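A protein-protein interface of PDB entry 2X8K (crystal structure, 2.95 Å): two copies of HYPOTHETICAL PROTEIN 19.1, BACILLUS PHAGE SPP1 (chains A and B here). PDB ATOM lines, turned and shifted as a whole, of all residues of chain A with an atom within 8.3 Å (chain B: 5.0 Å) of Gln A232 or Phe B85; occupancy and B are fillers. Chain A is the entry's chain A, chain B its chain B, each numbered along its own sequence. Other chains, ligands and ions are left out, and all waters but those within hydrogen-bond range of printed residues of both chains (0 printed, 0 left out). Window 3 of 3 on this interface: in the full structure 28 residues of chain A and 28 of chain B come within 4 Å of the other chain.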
ATOM      1  N   VAL A  33     -13.913  16.991  10.753  1.00  0.00           N
ATOM      2  CA  VAL A  33     -13.108  17.187   9.568  1.00  0.00           C
ATOM      3  C   VAL A  33     -13.340  18.546   8.942  1.00  0.00           C
ATOM      4  O   VAL A  33     -14.426  18.839   8.460  1.00  0.00           O
ATOM      5  CB  VAL A  33     -13.258  15.997   8.580  1.00  0.00           C
ATOM      6  CG1 VAL A  33     -12.174  16.050   7.508  1.00  0.00           C
ATOM      7  CG2 VAL A  33     -13.231  14.658   9.316  1.00  0.00           C
ATOM      8  N   TYR A  34     -12.340  19.401   9.030  1.00  0.00           N
ATOM      9  CA  TYR A  34     -12.430  20.761   8.507  1.00  0.00           C
ATOM     10  C   TYR A  34     -12.504  20.790   6.997  1.00  0.00           C
ATOM     11  O   TYR A  34     -11.897  19.934   6.346  1.00  0.00           O
ATOM     12  CB  TYR A  34     -11.269  21.617   9.016  1.00  0.00           C
ATOM     13  CG  TYR A  34     -11.704  23.025   9.340  1.00  0.00           C
ATOM     14  CD1 TYR A  34     -12.366  23.317  10.528  1.00  0.00           C
ATOM     15  CD2 TYR A  34     -11.433  24.075   8.467  1.00  0.00           C
ATOM     16  CE1 TYR A  34     -12.766  24.615  10.829  1.00  0.00           C
ATOM     17  CE2 TYR A  34     -11.796  25.381   8.771  1.00  0.00           C
ATOM     18  CZ  TYR A  34     -12.472  25.645   9.947  1.00  0.00           C
ATOM     19  OH  TYR A  34     -12.854  26.933  10.227  1.00  0.00           O
ATOM     20  N   VAL A 151      14.421  21.757  16.786  1.00  0.00           N
ATOM     21  CA  VAL A 151      13.252  22.141  17.570  1.00  0.00           C
ATOM     22  C   VAL A 151      12.112  21.533  16.817  1.00  0.00           C
ATOM     23  O   VAL A 151      11.939  21.846  15.644  1.00  0.00           O
ATOM     24  CB  VAL A 151      13.112  23.677  17.730  1.00  0.00           C
ATOM     25  CG1 VAL A 151      11.809  24.032  18.432  1.00  0.00           C
ATOM     26  CG2 VAL A 151      14.320  24.273  18.477  1.00  0.00           C
ATOM     27  N   LYS A 152      11.404  20.596  17.437  1.00  0.00           N
ATOM     28  CA  LYS A 152      10.302  19.901  16.770  1.00  0.00           C
ATOM     29  C   LYS A 152       8.971  20.504  17.145  1.00  0.00           C
ATOM     30  O   LYS A 152       8.656  20.596  18.334  1.00  0.00           O
ATOM     31  CB  LYS A 152      10.353  18.386  17.073  1.00  0.00           C
ATOM     32  CG  LYS A 152       9.023  17.638  16.990  1.00  0.00           C
ATOM     33  CD  LYS A 152       8.823  16.948  15.661  1.00  0.00           C
ATOM     34  CE  LYS A 152       7.989  15.704  15.834  1.00  0.00           C
ATOM     35  NZ  LYS A 152       8.769  14.656  16.552  1.00  0.00           N
ATOM     36  N   ASN A 153       8.193  20.920  16.142  1.00  0.00           N
ATOM     37  CA  ASN A 153       6.867  21.465  16.401  1.00  0.00           C
ATOM     38  C   ASN A 153       5.888  20.288  16.569  1.00  0.00           C
ATOM     39  O   ASN A 153       5.489  19.657  15.588  1.00  0.00           O
ATOM     40  CB  ASN A 153       6.449  22.446  15.297  1.00  0.00           C
ATOM     41  CG  ASN A 153       4.981  22.799  15.225  1.00  0.00           C
ATOM     42  OD1 ASN A 153       4.211  22.576  16.150  1.00  0.00           O
ATOM     43  ND2 ASN A 153       4.572  23.377  14.108  1.00  0.00           N
ATOM     44  N   THR A 154       5.526  20.004  17.826  1.00  0.00           N
ATOM     45  CA  THR A 154       4.635  18.917  18.230  1.00  0.00           C
ATOM     46  C   THR A 154       3.145  19.099  17.881  1.00  0.00           C
ATOM     47  O   THR A 154       2.378  18.137  17.963  1.00  0.00           O
ATOM     48  CB  THR A 154       4.920  18.500  19.668  1.00  0.00           C
ATOM     49  OG1 THR A 154       5.125  19.667  20.470  1.00  0.00           O
ATOM     50  CG2 THR A 154       6.142  17.605  19.757  1.00  0.00           C
ATOM     51  N   GLY A 155       2.765  20.301  17.445  1.00  0.00           N
ATOM     52  CA  GLY A 155       1.409  20.612  17.001  1.00  0.00           C
ATOM     53  C   GLY A 155       1.158  20.014  15.634  1.00  0.00           C
ATOM     54  O   GLY A 155       2.019  19.318  15.082  1.00  0.00           O
ATOM     55  N   LEU A 156      -0.019  20.277  15.066  1.00  0.00           N
ATOM     56  CA  LEU A 156      -0.342  19.743  13.754  1.00  0.00           C
ATOM     57  C   LEU A 156      -0.474  20.803  12.693  1.00  0.00           C
ATOM     58  O   LEU A 156      -0.679  20.476  11.528  1.00  0.00           O
ATOM     59  CB  LEU A 156      -1.542  18.805  13.797  1.00  0.00           C
ATOM     60  CG  LEU A 156      -1.330  17.490  14.532  1.00  0.00           C
ATOM     61  CD1 LEU A 156      -2.669  16.830  14.806  1.00  0.00           C
ATOM     62  CD2 LEU A 156      -0.354  16.546  13.779  1.00  0.00           C
ATOM     63  N   ALA A 157      -0.291  22.061  13.070  1.00  0.00           N
ATOM     64  CA  ALA A 157      -0.309  23.195  12.158  1.00  0.00           C
ATOM     65  C   ALA A 157       0.976  24.016  12.339  1.00  0.00           C
ATOM     66  O   ALA A 157       1.664  23.904  13.379  1.00  0.00           O
ATOM     67  CB  ALA A 157      -1.521  24.056  12.440  1.00  0.00           C
ATOM     68  N   VAL A 158       1.293  24.848  11.326  1.00  0.00           N
ATOM     69  CA  VAL A 158       2.443  25.751  11.361  1.00  0.00           C
ATOM     70  C   VAL A 158       2.226  26.757  12.509  1.00  0.00           C
ATOM     71  O   VAL A 158       1.104  27.227  12.728  1.00  0.00           O
ATOM     72  CB  VAL A 158       2.669  26.430   9.990  1.00  0.00           C
ATOM     73  CG1 VAL A 158       3.274  27.826  10.125  1.00  0.00           C
ATOM     74  CG2 VAL A 158       3.518  25.548   9.079  1.00  0.00           C
ATOM     75  N   LEU A 229       7.515  27.480  12.441  1.00  0.00           N
ATOM     76  CA  LEU A 229       7.823  26.088  12.755  1.00  0.00           C
ATOM     77  C   LEU A 229       6.812  25.152  12.057  1.00  0.00           C
ATOM     78  O   LEU A 229       5.628  25.195  12.391  1.00  0.00           O
ATOM     79  CB  LEU A 229       7.697  25.934  14.280  1.00  0.00           C
ATOM     80  CG  LEU A 229       8.938  25.964  15.165  1.00  0.00           C
ATOM     81  CD1 LEU A 229       9.903  27.051  14.777  1.00  0.00           C
ATOM     82  CD2 LEU A 229       8.539  26.178  16.581  1.00  0.00           C
ATOM     83  N   LYS A 230       7.265  24.334  11.073  1.00  0.00           N
ATOM     84  CA  LYS A 230       6.389  23.397  10.341  1.00  0.00           C
ATOM     85  C   LYS A 230       6.036  22.197  11.243  1.00  0.00           C
ATOM     86  O   LYS A 230       6.870  21.808  12.065  1.00  0.00           O
ATOM     87  CB  LYS A 230       7.027  22.912   9.027  1.00  0.00           C
ATOM     88  CG  LYS A 230       7.159  23.970   7.931  1.00  0.00           C
ATOM     89  CD  LYS A 230       7.820  23.366   6.680  1.00  0.00           C
ATOM     90  CE  LYS A 230       8.615  24.332   5.825  1.00  0.00           C
ATOM     91  NZ  LYS A 230       9.646  23.624   5.025  1.00  0.00           N
ATOM     92  N   PRO A 231       4.833  21.586  11.122  1.00  0.00           N
ATOM     93  CA  PRO A 231       4.479  20.497  12.057  1.00  0.00           C
ATOM     94  C   PRO A 231       5.110  19.131  11.818  1.00  0.00           C
ATOM     95  O   PRO A 231       5.473  18.807  10.686  1.00  0.00           O
ATOM     96  CB  PRO A 231       2.954  20.438  11.987  1.00  0.00           C
ATOM     97  CG  PRO A 231       2.617  21.009  10.697  1.00  0.00           C
ATOM     98  CD  PRO A 231       3.704  21.924  10.237  1.00  0.00           C
ATOM     99  N   GLN A 232       5.244  18.332  12.912  1.00  0.00           N
ATOM    100  CA  GLN A 232       5.739  16.949  12.933  1.00  0.00           C
ATOM    101  C   GLN A 232       7.119  16.787  12.302  1.00  0.00           C
ATOM    102  O   GLN A 232       7.522  15.684  11.896  1.00  0.00           O
ATOM    103  CB  GLN A 232       4.701  16.020  12.259  1.00  0.00           C
ATOM    104  CG  GLN A 232       3.306  16.101  12.864  1.00  0.00           C
ATOM    105  CD  GLN A 232       3.346  15.792  14.331  1.00  0.00           C
ATOM    106  OE1 GLN A 232       3.594  14.662  14.732  1.00  0.00           O
ATOM    107  NE2 GLN A 232       3.172  16.800  15.167  1.00  0.00           N
ATOM    108  N   VAL A 233       7.845  17.915  12.247  1.00  0.00           N
ATOM    109  CA  VAL A 233       9.143  18.069  11.608  1.00  0.00           C
ATOM    110  C   VAL A 233      10.085  18.971  12.443  1.00  0.00           C
ATOM    111  O   VAL A 233       9.631  19.949  13.067  1.00  0.00           O
ATOM    112  CB  VAL A 233       8.843  18.614  10.178  1.00  0.00           C
ATOM    113  CG1 VAL A 233       9.945  19.518   9.629  1.00  0.00           C
ATOM    114  CG2 VAL A 233       8.509  17.481   9.211  1.00  0.00           C
ATOM    115  N   ASN A 234      11.396  18.634  12.437  1.00  0.00           N
ATOM    116  CA  ASN A 234      12.439  19.399  13.125  1.00  0.00           C
ATOM    117  C   ASN A 234      12.748  20.700  12.405  1.00  0.00           C
ATOM    118  O   ASN A 234      12.785  20.739  11.174  1.00  0.00           O
ATOM    119  CB  ASN A 234      13.731  18.588  13.248  1.00  0.00           C
ATOM    120  CG  ASN A 234      13.754  17.601  14.391  1.00  0.00           C
ATOM    121  OD1 ASN A 234      13.289  17.871  15.500  1.00  0.00           O
ATOM    122  ND2 ASN A 234      14.339  16.442  14.161  1.00  0.00           N
ATOM    123  N   THR A 235      12.990  21.755  13.189  1.00  0.00           N
ATOM    124  CA  THR A 235      13.365  23.091  12.737  1.00  0.00           C
ATOM    125  C   THR A 235      14.727  23.363  13.378  1.00  0.00           C
ATOM    126  O   THR A 235      14.847  23.314  14.607  1.00  0.00           O
ATOM    127  CB  THR A 235      12.283  24.116  13.125  1.00  0.00           C
ATOM    128  OG1 THR A 235      11.037  23.773  12.502  1.00  0.00           O
ATOM    129  CG2 THR A 235      12.659  25.533  12.748  1.00  0.00           C
ATOM    130  N   GLU A 249       1.573  24.784  20.372  1.00  0.00           N
ATOM    131  CA  GLU A 249       1.026  23.718  19.526  1.00  0.00           C
ATOM    132  C   GLU A 249      -0.329  24.183  18.999  1.00  0.00           C
ATOM    133  O   GLU A 249      -1.103  24.768  19.775  1.00  0.00           O
ATOM    134  CB  GLU A 249       0.823  22.427  20.348  1.00  0.00           C
ATOM    135  CG  GLU A 249       2.080  21.743  20.861  1.00  0.00           C
ATOM    136  CD  GLU A 249       1.847  20.472  21.658  1.00  0.00           C
ATOM    137  OE1 GLU A 249       0.669  20.128  21.910  1.00  0.00           O
ATOM    138  OE2 GLU A 249       2.848  19.824  22.045  1.00  0.00           O
ATOM    139  N   LYS A 250      -0.606  23.963  17.686  1.00  0.00           N
ATOM    140  CA  LYS A 250      -1.885  24.357  17.051  1.00  0.00           C
ATOM    141  C   LYS A 250      -2.485  23.229  16.222  1.00  0.00           C
ATOM    142  O   LYS A 250      -1.747  22.435  15.644  1.00  0.00           O
ATOM    143  CB  LYS A 250      -1.720  25.598  16.181  1.00  0.00           C
ATOM    144  CG  LYS A 250      -1.724  26.895  16.942  1.00  0.00           C
ATOM    145  CD  LYS A 250      -0.915  27.943  16.193  1.00  0.00           C
ATOM    146  CE  LYS A 250      -1.502  28.382  14.849  1.00  0.00           C
ATOM    147  NZ  LYS A 250      -2.652  29.335  14.979  1.00  0.00           N
ATOM    148  N   PHE A 251      -3.821  23.150  16.165  1.00  0.00           N
ATOM    149  CA  PHE A 251      -4.498  22.064  15.462  1.00  0.00           C
ATOM    150  C   PHE A 251      -5.713  22.579  14.735  1.00  0.00           C
ATOM    151  O   PHE A 251      -6.313  23.547  15.208  1.00  0.00           O
ATOM    152  CB  PHE A 251      -4.947  20.999  16.478  1.00  0.00           C
ATOM    153  CG  PHE A 251      -3.887  20.618  17.474  1.00  0.00           C
ATOM    154  CD1 PHE A 251      -3.016  19.570  17.215  1.00  0.00           C
ATOM    155  CD2 PHE A 251      -3.724  21.341  18.655  1.00  0.00           C
ATOM    156  CE1 PHE A 251      -2.016  19.233  18.131  1.00  0.00           C
ATOM    157  CE2 PHE A 251      -2.699  21.033  19.538  1.00  0.00           C
ATOM    158  CZ  PHE A 251      -1.865  19.966  19.282  1.00  0.00           C
ATOM    159  N   LEU A 252      -6.118  21.913  13.623  1.00  0.00           N
ATOM    160  CA  LEU A 252      -7.356  22.257  12.904  1.00  0.00           C
ATOM    161  C   LEU A 252      -8.591  21.429  13.403  1.00  0.00           C
ATOM    162  O   LEU A 252      -9.682  22.017  13.528  1.00  0.00           O
ATOM    163  CB  LEU A 252      -7.218  22.112  11.363  1.00  0.00           C
ATOM    164  CG  LEU A 252      -7.574  23.319  10.479  1.00  0.00           C
ATOM    165  CD1 LEU A 252      -7.880  22.886   9.111  1.00  0.00           C
ATOM    166  CD2 LEU A 252      -8.781  24.113  11.000  1.00  0.00           C
ATOM    167  OXT LEU A 252      -8.493  20.191  13.581  1.00  0.00           O
ATOM    168  N   GLU B  81      -8.277  15.590  14.486  1.00  0.00           N
ATOM    169  CA  GLU B  81      -7.263  16.638  14.362  1.00  0.00           C
ATOM    170  C   GLU B  81      -6.142  16.136  13.442  1.00  0.00           C
ATOM    171  O   GLU B  81      -5.690  16.864  12.554  1.00  0.00           O
ATOM    172  CB  GLU B  81      -6.652  16.954  15.744  1.00  0.00           C
ATOM    173  CG  GLU B  81      -7.411  17.950  16.594  1.00  0.00           C
ATOM    174  CD  GLU B  81      -6.929  18.075  18.020  1.00  0.00           C
ATOM    175  OE1 GLU B  81      -5.753  17.721  18.265  1.00  0.00           O
ATOM    176  OE2 GLU B  81      -7.719  18.517  18.891  1.00  0.00           O
ATOM    177  N   TYR B  82      -5.714  14.878  13.665  1.00  0.00           N
ATOM    178  CA  TYR B  82      -4.678  14.230  12.889  1.00  0.00           C
ATOM    179  C   TYR B  82      -5.160  13.971  11.494  1.00  0.00           C
ATOM    180  O   TYR B  82      -4.406  14.180  10.549  1.00  0.00           O
ATOM    181  CB  TYR B  82      -4.187  12.940  13.564  1.00  0.00           C
ATOM    182  CG  TYR B  82      -2.855  12.487  13.000  1.00  0.00           C
ATOM    183  CD1 TYR B  82      -1.678  13.185  13.286  1.00  0.00           C
ATOM    184  CD2 TYR B  82      -2.780  11.425  12.101  1.00  0.00           C
ATOM    185  CE1 TYR B  82      -0.468  12.843  12.682  1.00  0.00           C
ATOM    186  CE2 TYR B  82      -1.571  11.063  11.512  1.00  0.00           C
ATOM    187  CZ  TYR B  82      -0.419  11.776  11.802  1.00  0.00           C
ATOM    188  OH  TYR B  82       0.779  11.400  11.237  1.00  0.00           O
ATOM    189  N   LEU B  83      -6.435  13.574  11.346  1.00  0.00           N
ATOM    190  CA  LEU B  83      -7.051  13.302  10.043  1.00  0.00           C
ATOM    191  C   LEU B  83      -7.019  14.557   9.222  1.00  0.00           C
ATOM    192  O   LEU B  83      -6.706  14.484   8.045  1.00  0.00           O
ATOM    193  CB  LEU B  83      -8.498  12.862  10.238  1.00  0.00           C
ATOM    194  CG  LEU B  83      -9.055  11.760   9.346  1.00  0.00           C
ATOM    195  CD1 LEU B  83     -10.502  12.047   8.998  1.00  0.00           C
ATOM    196  CD2 LEU B  83      -8.230  11.524   8.078  1.00  0.00           C
ATOM    197  N   ASN B  84      -7.274  15.728   9.866  1.00  0.00           N
ATOM    198  CA  ASN B  84      -7.212  17.035   9.202  1.00  0.00           C
ATOM    199  C   ASN B  84      -5.798  17.307   8.707  1.00  0.00           C
ATOM    200  O   ASN B  84      -5.622  17.761   7.572  1.00  0.00           O
ATOM    201  CB  ASN B  84      -7.695  18.133  10.108  1.00  0.00           C
ATOM    202  CG  ASN B  84      -9.189  18.197  10.169  1.00  0.00           C
ATOM    203  OD1 ASN B  84      -9.878  18.158   9.146  1.00  0.00           O
ATOM    204  ND2 ASN B  84      -9.734  18.280  11.363  1.00  0.00           N
ATOM    205  N   PHE B  85      -4.792  16.934   9.531  1.00  0.00           N
ATOM    206  CA  PHE B  85      -3.375  17.063   9.213  1.00  0.00           C
ATOM    207  C   PHE B  85      -2.995  16.298   7.946  1.00  0.00           C
ATOM    208  O   PHE B  85      -2.303  16.846   7.073  1.00  0.00           O
ATOM    209  CB  PHE B  85      -2.524  16.639  10.406  1.00  0.00           C
ATOM    210  CG  PHE B  85      -1.057  16.490  10.115  1.00  0.00           C
ATOM    211  CD1 PHE B  85      -0.247  17.614   9.941  1.00  0.00           C
ATOM    212  CD2 PHE B  85      -0.465  15.224  10.070  1.00  0.00           C
ATOM    213  CE1 PHE B  85       1.125  17.474   9.720  1.00  0.00           C
ATOM    214  CE2 PHE B  85       0.897  15.079   9.799  1.00  0.00           C
ATOM    215  CZ  PHE B  85       1.684  16.205   9.630  1.00  0.00           C
ATOM    216  N   LEU B  86      -3.479  15.053   7.842  1.00  0.00           N
ATOM    217  CA  LEU B  86      -3.226  14.189   6.689  1.00  0.00           C
ATOM    218  C   LEU B  86      -3.954  14.654   5.418  1.00  0.00           C
ATOM    219  O   LEU B  86      -3.448  14.442   4.319  1.00  0.00           O
ATOM    220  CB  LEU B  86      -3.644  12.743   6.995  1.00  0.00           C
ATOM    221  CG  LEU B  86      -3.002  12.094   8.193  1.00  0.00           C
ATOM    222  CD1 LEU B  86      -3.631  10.761   8.484  1.00  0.00           C
ATOM    223  CD2 LEU B  86      -1.529  11.971   8.012  1.00  0.00           C
ATOM    224  N   LEU B  87      -5.138  15.254   5.571  1.00  0.00           N
ATOM    225  CA  LEU B  87      -5.959  15.663   4.452  1.00  0.00           C
ATOM    226  C   LEU B  87      -5.644  16.999   3.827  1.00  0.00           C
ATOM    227  O   LEU B  87      -5.716  17.082   2.609  1.00  0.00           O
ATOM    228  CB  LEU B  87      -7.451  15.587   4.804  1.00  0.00           C
ATOM    229  CG  LEU B  87      -8.039  14.212   5.049  1.00  0.00           C
ATOM    230  CD1 LEU B  87      -9.333  14.323   5.798  1.00  0.00           C
ATOM    231  CD2 LEU B  87      -8.209  13.422   3.744  1.00  0.00           C
ATOM    232  N   HIS B  88      -5.393  18.063   4.613  1.00  0.00           N
ATOM    233  CA  HIS B  88      -5.169  19.398   4.043  1.00  0.00           C
ATOM    234  C   HIS B  88      -3.893  19.460   3.227  1.00  0.00           C
ATOM    235  O   HIS B  88      -2.795  19.240   3.750  1.00  0.00           O
ATOM    236  CB  HIS B  88      -5.322  20.538   5.081  1.00  0.00           C
ATOM    237  CG  HIS B  88      -5.154  21.948   4.548  1.00  0.00           C
ATOM    238  ND1 HIS B  88      -4.440  22.905   5.259  1.00  0.00           N
ATOM    239  CD2 HIS B  88      -5.639  22.533   3.422  1.00  0.00           C
ATOM    240  CE1 HIS B  88      -4.513  24.023   4.545  1.00  0.00           C
ATOM    241  NE2 HIS B  88      -5.211  23.850   3.427  1.00  0.00           N
ATOM    242  N   ARG B  89      -4.074  19.682   1.913  1.00  0.00           N
ATOM    243  CA  ARG B  89      -3.027  19.744   0.908  1.00  0.00           C
ATOM    244  C   ARG B  89      -3.219  20.968   0.022  1.00  0.00           C
ATOM    245  O   ARG B  89      -4.347  21.283  -0.351  1.00  0.00           O
ATOM    246  CB  ARG B  89      -3.097  18.476   0.068  1.00  0.00           C
ATOM    247  CG  ARG B  89      -1.742  17.884  -0.209  1.00  0.00           C
ATOM    248  CD  ARG B  89      -1.423  16.657   0.623  1.00  0.00           C
ATOM    249  NE  ARG B  89      -1.405  16.900   2.063  1.00  0.00           N
ATOM    250  CZ  ARG B  89      -0.841  16.071   2.935  1.00  0.00           C
ATOM    251  NH1 ARG B  89      -0.210  14.986   2.511  1.00  0.00           N
ATOM    252  NH2 ARG B  89      -0.901  16.325   4.238  1.00  0.00           N
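N of Tyr A34 lies within hydrogen-bond range of OD1 of Asn B84.
ND2 of Asn B84 sits at hydrogen-bond distance from OXT of Leu A252.
The backbone carbonyl oxygen of Asn A153 sits at hydrogen-bond distance from the backbone NH of Gln A232.
NE2 of Gln A232 sits at hydrogen-bond distance from O of Thr A154 (3.2 Å).
The backbone carbonyl oxygen (O) of Gly A155 lies within hydrogen-bond range of the side-chain amide nitrogen (NE2) of Gln A232, at 2.8 Å.
N of Leu A156 is in hydrogen-bond range of O of Lys A250, at 2.8 Å.
The guanidinium group of Arg B89 lies within hydrogen-bond range of the backbone carbonyl oxygen of Phe B85 (3.2 Å).
CD1 of Leu B83 touches CG2 of Val A33, 3.8 Å away.
CA of Val A33 touches OD1 of Asn B84 (3.4 Å).
Val A33 touches Leu B87 (CG1 to CD1, 3.7 Å).
Leu A156 touches Glu B81 (CD1 to O, 3.8 Å).
Leu A156 touches Tyr B82.
O of Leu A156 touches CD1 of Phe B85, at 3.3 Å.
Pro A231 touches Phe B85.
Gln A232 touches Phe B85.
Phe A251 touches Glu B81 (CD1 to OE1, 3.5 Å).
Glu B81 touches Leu A252.
Gln A232 touches one residue of chain B.
Phe B85 touches three residues of chain A.
Of the printed residues of chain A, Tyr B82 touches Leu A156.
Printed residues of chain A within 4 Å of Leu B83: Val A33 (3.8 Å).
Of the printed residues of chain B, Leu A252 touches Glu B81 and Asn B84.
Of the printed residues of chain B, Phe A251 touches Glu B81 (3.5 Å).
Printed residues of chain B within 4 Å of Pro A231: Phe B85 (3.96 Å).
Gly A155 touches none of the printed residues of chain B.
Lys A152 touches none of the printed residues of chain B.
The nearest printed residue of chain A that does not touch Tyr B82 is Gln A232 (4.9 Å).
Along chain B the printed residues that touch a printed residue of chain A span positions 81 to 87.
Among the printed residues, no Asp or Glu carboxylate lies within 4 Å of a Lys or Arg side-chain nitrogen of the other chain.
No position is printed for both chains.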
